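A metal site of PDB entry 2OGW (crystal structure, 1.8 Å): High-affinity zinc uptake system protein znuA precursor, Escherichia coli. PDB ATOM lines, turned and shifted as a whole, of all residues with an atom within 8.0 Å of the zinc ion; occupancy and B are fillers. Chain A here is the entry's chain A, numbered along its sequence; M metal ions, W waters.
A ring nitrogen (ND1) of His 207 lies within hydrogen-bond range of the side-chain carboxylate (OE1) of Glu 256.
OG of Ser 58 sits close to N of His 60.
The backbone NH (N) of His 143 is in hydrogen-bond range of the side-chain amide oxygen (OD1) of Asn 141, at 2.9 Å.
A ring nitrogen (ND1) of His 143 sits close to the backbone carbonyl oxygen of Asp 208, at 3.4 Å.
OE2 of Glu 59 touches the zinc ion, at 3.9 Å.
Of the 20 residues printed, 4 come within 4 Å of the zinc ion.
Along chain A the residues within 4 Å of the zinc ion span positions 59 to 207.
The nearest printed residue that does not touch the zinc ion is Ala 209 (4.1 Å).
A ring nitrogen (NE2) of His 60 binds the zinc ion.
The zinc ion is bound by a ring nitrogen (NE2) of His 207 (2.0 Å).
NE2 of His 143 binds the zinc ion (2.1 Å).
The zinc ion is bound by water W1, 2.3 Å away.
The zinc ion has four donor atoms within binding distance.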
ATOM      1  N   LEU A  32     -14.077  18.570  -9.566  1.00  0.00           N
ATOM      2  CA  LEU A  32     -13.659  18.346  -8.203  1.00  0.00           C
ATOM      3  C   LEU A  32     -14.257  19.403  -7.323  1.00  0.00           C
ATOM      4  O   LEU A  32     -14.515  20.534  -7.794  1.00  0.00           O
ATOM      5  CB  LEU A  32     -12.129  18.445  -8.062  1.00  0.00           C
ATOM      6  CG  LEU A  32     -11.339  17.675  -9.073  1.00  0.00           C
ATOM      7  CD1 LEU A  32      -9.917  18.147  -9.058  1.00  0.00           C
ATOM      8  CD2 LEU A  32     -11.496  16.145  -8.826  1.00  0.00           C
ATOM      9  N   SER A  58     -11.134  10.341  -4.341  1.00  0.00           N
ATOM     10  CA  SER A  58      -9.906  11.047  -4.708  1.00  0.00           C
ATOM     11  C   SER A  58      -9.729  11.161  -6.226  1.00  0.00           C
ATOM     12  O   SER A  58      -9.873  10.145  -6.907  1.00  0.00           O
ATOM     13  CB  SER A  58      -8.697  10.294  -4.119  1.00  0.00           C
ATOM     14  OG  SER A  58      -7.441  10.772  -4.639  1.00  0.00           O
ATOM     15  N   GLU A  59      -9.364  12.355  -6.717  1.00  0.00           N
ATOM     16  CA  GLU A  59      -9.007  12.586  -8.163  1.00  0.00           C
ATOM     17  C   GLU A  59      -7.924  11.669  -8.668  1.00  0.00           C
ATOM     18  O   GLU A  59      -7.729  11.583  -9.875  1.00  0.00           O
ATOM     19  CB  GLU A  59      -8.527  14.034  -8.463  1.00  0.00           C
ATOM     20  CG  GLU A  59      -7.593  14.627  -7.428  1.00  0.00           C
ATOM     21  CD  GLU A  59      -8.297  14.776  -6.121  1.00  0.00           C
ATOM     22  OE1 GLU A  59      -9.515  15.054  -6.185  1.00  0.00           O
ATOM     23  OE2 GLU A  59      -7.671  14.576  -5.044  1.00  0.00           O
ATOM     24  N   HIS A  60      -7.194  11.023  -7.763  1.00  0.00           N
ATOM     25  CA  HIS A  60      -6.121  10.112  -8.196  1.00  0.00           C
ATOM     26  C   HIS A  60      -6.583   8.663  -8.402  1.00  0.00           C
ATOM     27  O   HIS A  60      -5.770   7.805  -8.838  1.00  0.00           O
ATOM     28  CB  HIS A  60      -4.986  10.142  -7.181  1.00  0.00           C
ATOM     29  CG  HIS A  60      -4.432  11.500  -6.979  1.00  0.00           C
ATOM     30  ND1 HIS A  60      -3.592  12.088  -7.908  1.00  0.00           N
ATOM     31  CD2 HIS A  60      -4.631  12.428  -6.012  1.00  0.00           C
ATOM     32  CE1 HIS A  60      -3.257  13.297  -7.491  1.00  0.00           C
ATOM     33  NE2 HIS A  60      -3.888  13.525  -6.356  1.00  0.00           N
ATOM     34  N   MET A  85      -4.443  15.863 -14.955  1.00  0.00           N
ATOM     35  CA  MET A  85      -5.032  15.705 -13.633  1.00  0.00           C
ATOM     36  C   MET A  85      -6.147  14.646 -13.781  1.00  0.00           C
ATOM     37  O   MET A  85      -5.895  13.446 -13.599  1.00  0.00           O
ATOM     38  CB  MET A  85      -5.535  17.079 -13.093  1.00  0.00           C
ATOM     39  CG  MET A  85      -6.156  17.060 -11.709  1.00  0.00           C
ATOM     40  SD  MET A  85      -5.039  16.121 -10.361  1.00  0.00           S
ATOM     41  CE  MET A  85      -3.977  17.315  -9.823  1.00  0.00           C
ATOM     42  N   ASN A 141       2.968  20.409 -11.347  1.00  0.00           N
ATOM     43  CA  ASN A 141       2.050  20.081 -10.259  1.00  0.00           C
ATOM     44  C   ASN A 141       0.679  20.521 -10.732  1.00  0.00           C
ATOM     45  O   ASN A 141       0.513  21.680 -11.094  1.00  0.00           O
ATOM     46  CB  ASN A 141       2.422  20.906  -9.035  1.00  0.00           C
ATOM     47  CG  ASN A 141       1.472  20.702  -7.870  1.00  0.00           C
ATOM     48  OD1 ASN A 141       0.416  20.049  -7.956  1.00  0.00           O
ATOM     49  ND2 ASN A 141       1.870  21.279  -6.737  1.00  0.00           N
ATOM     50  N   MET A 142      -0.300  19.618 -10.703  1.00  0.00           N
ATOM     51  CA  MET A 142      -1.630  19.936 -11.251  1.00  0.00           C
ATOM     52  C   MET A 142      -2.695  20.239 -10.195  1.00  0.00           C
ATOM     53  O   MET A 142      -3.906  20.271 -10.479  1.00  0.00           O
ATOM     54  CB  MET A 142      -2.079  18.783 -12.193  1.00  0.00           C
ATOM     55  CG  MET A 142      -1.400  18.780 -13.506  1.00  0.00           C
ATOM     56  SD  MET A 142      -2.014  20.207 -14.666  1.00  0.00           S
ATOM     57  CE  MET A 142      -0.327  20.777 -15.535  1.00  0.00           C
ATOM     58  N   HIS A 143      -2.238  20.454  -8.956  1.00  0.00           N
ATOM     59  CA  HIS A 143      -3.144  20.790  -7.849  1.00  0.00           C
ATOM     60  C   HIS A 143      -3.476  22.286  -7.887  1.00  0.00           C
ATOM     61  O   HIS A 143      -3.230  23.040  -6.934  1.00  0.00           O
ATOM     62  CB  HIS A 143      -2.558  20.303  -6.503  1.00  0.00           C
ATOM     63  CG  HIS A 143      -2.483  18.809  -6.406  1.00  0.00           C
ATOM     64  ND1 HIS A 143      -1.454  18.101  -6.971  1.00  0.00           N
ATOM     65  CD2 HIS A 143      -3.309  17.901  -5.835  1.00  0.00           C
ATOM     66  CE1 HIS A 143      -1.645  16.804  -6.754  1.00  0.00           C
ATOM     67  NE2 HIS A 143      -2.748  16.667  -6.052  1.00  0.00           N
ATOM     68  N   TRP A 145      -6.175  24.127  -7.975  1.00  0.00           N
ATOM     69  CA  TRP A 145      -7.295  24.811  -7.286  1.00  0.00           C
ATOM     70  C   TRP A 145      -6.857  25.394  -5.953  1.00  0.00           C
ATOM     71  O   TRP A 145      -7.638  26.137  -5.319  1.00  0.00           O
ATOM     72  CB  TRP A 145      -8.490  23.874  -7.048  1.00  0.00           C
ATOM     73  CG  TRP A 145      -8.125  22.614  -6.296  1.00  0.00           C
ATOM     74  CD1 TRP A 145      -8.171  22.406  -4.934  1.00  0.00           C
ATOM     75  CD2 TRP A 145      -7.639  21.386  -6.872  1.00  0.00           C
ATOM     76  NE1 TRP A 145      -7.734  21.115  -4.636  1.00  0.00           N
ATOM     77  CE2 TRP A 145      -7.400  20.476  -5.798  1.00  0.00           C
ATOM     78  CE3 TRP A 145      -7.363  20.980  -8.170  1.00  0.00           C
ATOM     79  CZ2 TRP A 145      -6.920  19.172  -6.015  1.00  0.00           C
ATOM     80  CZ3 TRP A 145      -6.921  19.659  -8.394  1.00  0.00           C
ATOM     81  CH2 TRP A 145      -6.673  18.782  -7.295  1.00  0.00           C
ATOM     82  N   HIS A 207       0.179  13.436   0.786  1.00  0.00           N
ATOM     83  CA  HIS A 207       0.574  13.531  -0.632  1.00  0.00           C
ATOM     84  C   HIS A 207       0.768  14.966  -1.076  1.00  0.00           C
ATOM     85  O   HIS A 207       0.333  15.923  -0.430  1.00  0.00           O
ATOM     86  CB  HIS A 207      -0.319  12.701  -1.624  1.00  0.00           C
ATOM     87  CG  HIS A 207      -1.480  13.430  -2.255  1.00  0.00           C
ATOM     88  ND1 HIS A 207      -2.665  13.673  -1.583  1.00  0.00           N
ATOM     89  CD2 HIS A 207      -1.663  13.931  -3.508  1.00  0.00           C
ATOM     90  CE1 HIS A 207      -3.535  14.260  -2.391  1.00  0.00           C
ATOM     91  NE2 HIS A 207      -2.952  14.458  -3.552  1.00  0.00           N
ATOM     92  N   ASP A 208       1.463  15.069  -2.200  1.00  0.00           N
ATOM     93  CA  ASP A 208       1.996  16.319  -2.689  1.00  0.00           C
ATOM     94  C   ASP A 208       0.910  17.152  -3.400  1.00  0.00           C
ATOM     95  O   ASP A 208       0.934  17.290  -4.632  1.00  0.00           O
ATOM     96  CB  ASP A 208       3.167  15.989  -3.612  1.00  0.00           C
ATOM     97  CG  ASP A 208       3.967  17.189  -4.007  1.00  0.00           C
ATOM     98  OD1 ASP A 208       3.841  18.223  -3.310  1.00  0.00           O
ATOM     99  OD2 ASP A 208       4.698  17.103  -5.016  1.00  0.00           O
ATOM    100  N   ALA A 209      -0.044  17.657  -2.625  1.00  0.00           N
ATOM    101  CA  ALA A 209      -1.215  18.379  -3.135  1.00  0.00           C
ATOM    102  C   ALA A 209      -1.157  19.902  -2.877  1.00  0.00           C
ATOM    103  O   ALA A 209      -1.975  20.629  -3.417  1.00  0.00           O
ATOM    104  CB  ALA A 209      -2.472  17.829  -2.523  1.00  0.00           C
ATOM    105  N   TYR A 210      -0.257  20.341  -2.008  1.00  0.00           N
ATOM    106  CA  TYR A 210      -0.416  21.658  -1.379  1.00  0.00           C
ATOM    107  C   TYR A 210       0.543  22.729  -1.888  1.00  0.00           C
ATOM    108  O   TYR A 210       0.470  23.873  -1.391  1.00  0.00           O
ATOM    109  CB  TYR A 210      -0.336  21.524   0.175  1.00  0.00           C
ATOM    110  CG  TYR A 210      -1.233  20.399   0.645  1.00  0.00           C
ATOM    111  CD1 TYR A 210      -2.554  20.634   0.963  1.00  0.00           C
ATOM    112  CD2 TYR A 210      -0.754  19.079   0.722  1.00  0.00           C
ATOM    113  CE1 TYR A 210      -3.402  19.556   1.377  1.00  0.00           C
ATOM    114  CE2 TYR A 210      -1.575  18.038   1.086  1.00  0.00           C
ATOM    115  CZ  TYR A 210      -2.875  18.279   1.443  1.00  0.00           C
ATOM    116  OH  TYR A 210      -3.672  17.179   1.792  1.00  0.00           O
ATOM    117  N   VAL A 227       3.646  10.709  -3.627  1.00  0.00           N
ATOM    118  CA  VAL A 227       3.189  11.627  -4.719  1.00  0.00           C
ATOM    119  C   VAL A 227       1.763  11.228  -5.129  1.00  0.00           C
ATOM    120  O   VAL A 227       0.809  12.027  -5.039  1.00  0.00           O
ATOM    121  CB  VAL A 227       4.156  11.677  -5.923  1.00  0.00           C
ATOM    122  CG1 VAL A 227       3.576  12.488  -7.073  1.00  0.00           C
ATOM    123  CG2 VAL A 227       5.488  12.301  -5.470  1.00  0.00           C
ATOM    124  N   ASN A 228       1.617   9.975  -5.557  1.00  0.00           N
ATOM    125  CA  ASN A 228       0.310   9.383  -5.769  1.00  0.00           C
ATOM    126  C   ASN A 228      -0.102   8.660  -4.497  1.00  0.00           C
ATOM    127  O   ASN A 228       0.524   7.661  -4.121  1.00  0.00           O
ATOM    128  CB  ASN A 228       0.341   8.429  -6.961  1.00  0.00           C
ATOM    129  CG  ASN A 228      -1.050   7.965  -7.380  1.00  0.00           C
ATOM    130  OD1 ASN A 228      -1.979   7.961  -6.591  1.00  0.00           O
ATOM    131  ND2 ASN A 228      -1.174   7.548  -8.626  1.00  0.00           N
ATOM    132  N   PRO A 229      -1.165   9.160  -3.823  1.00  0.00           N
ATOM    133  CA  PRO A 229      -1.625   8.593  -2.556  1.00  0.00           C
ATOM    134  C   PRO A 229      -2.217   7.195  -2.744  1.00  0.00           C
ATOM    135  O   PRO A 229      -2.537   6.542  -1.755  1.00  0.00           O
ATOM    136  CB  PRO A 229      -2.709   9.578  -2.097  1.00  0.00           C
ATOM    137  CG  PRO A 229      -3.217  10.166  -3.365  1.00  0.00           C
ATOM    138  CD  PRO A 229      -2.003  10.325  -4.228  1.00  0.00           C
ATOM    139  N   GLU A 256      -4.946  12.704   5.486  1.00  0.00           N
ATOM    140  CA  GLU A 256      -6.036  13.291   4.640  1.00  0.00           C
ATOM    141  C   GLU A 256      -7.274  12.396   4.772  1.00  0.00           C
ATOM    142  O   GLU A 256      -7.132  11.195   4.974  1.00  0.00           O
ATOM    143  CB  GLU A 256      -5.609  13.392   3.175  1.00  0.00           C
ATOM    144  CG  GLU A 256      -4.327  14.278   3.039  1.00  0.00           C
ATOM    145  CD  GLU A 256      -3.561  14.117   1.745  1.00  0.00           C
ATOM    146  OE1 GLU A 256      -3.903  13.193   0.956  1.00  0.00           O
ATOM    147  OE2 GLU A 256      -2.547  14.851   1.577  1.00  0.00           O
ATOM    148  N   PHE A 259      -7.835   9.025   2.649  1.00  0.00           N
ATOM    149  CA  PHE A 259      -6.929   7.889   2.810  1.00  0.00           C
ATOM    150  C   PHE A 259      -6.815   7.473   4.265  1.00  0.00           C
ATOM    151  O   PHE A 259      -6.842   8.328   5.148  1.00  0.00           O
ATOM    152  CB  PHE A 259      -5.576   8.196   2.161  1.00  0.00           C
ATOM    153  CG  PHE A 259      -5.695   8.470   0.700  1.00  0.00           C
ATOM    154  CD1 PHE A 259      -5.841   7.434  -0.197  1.00  0.00           C
ATOM    155  CD2 PHE A 259      -5.776   9.778   0.234  1.00  0.00           C
ATOM    156  CE1 PHE A 259      -6.032   7.668  -1.556  1.00  0.00           C
ATOM    157  CE2 PHE A 259      -5.951  10.027  -1.115  1.00  0.00           C
ATOM    158  CZ  PHE A 259      -6.072   8.970  -2.017  1.00  0.00           C
ATOM    159  N   PRO A 280      -7.462  18.407   0.924  1.00  0.00           N
ATOM    160  CA  PRO A 280      -7.219  19.178  -0.298  1.00  0.00           C
ATOM    161  C   PRO A 280      -8.507  19.276  -1.176  1.00  0.00           C
ATOM    162  O   PRO A 280      -8.495  19.973  -2.181  1.00  0.00           O
ATOM    163  CB  PRO A 280      -6.090  18.405  -0.996  1.00  0.00           C
ATOM    164  CG  PRO A 280      -6.385  16.909  -0.607  1.00  0.00           C
ATOM    165  CD  PRO A 280      -6.899  17.031   0.838  1.00  0.00           C
ATOM    166  N   LEU A 281      -9.587  18.607  -0.797  1.00  0.00           N
ATOM    167  CA  LEU A 281     -10.812  18.575  -1.630  1.00  0.00           C
ATOM    168  C   LEU A 281     -12.026  19.201  -0.906  1.00  0.00           C
ATOM    169  O   LEU A 281     -13.152  19.126  -1.402  1.00  0.00           O
ATOM    170  CB  LEU A 281     -11.106  17.117  -2.033  1.00  0.00           C
ATOM    171  CG  LEU A 281     -10.126  16.513  -3.041  1.00  0.00           C
ATOM    172  CD1 LEU A 281     -10.586  15.054  -3.330  1.00  0.00           C
ATOM    173  CD2 LEU A 281     -10.031  17.388  -4.327  1.00  0.00           C
HETATM  174 ZN    ZN M   1      -3.813  15.075  -5.256  1.00  0.00          ZN
HETATM  175  O   HOH W   1      -5.771  15.871  -4.414  1.00  0.00           O
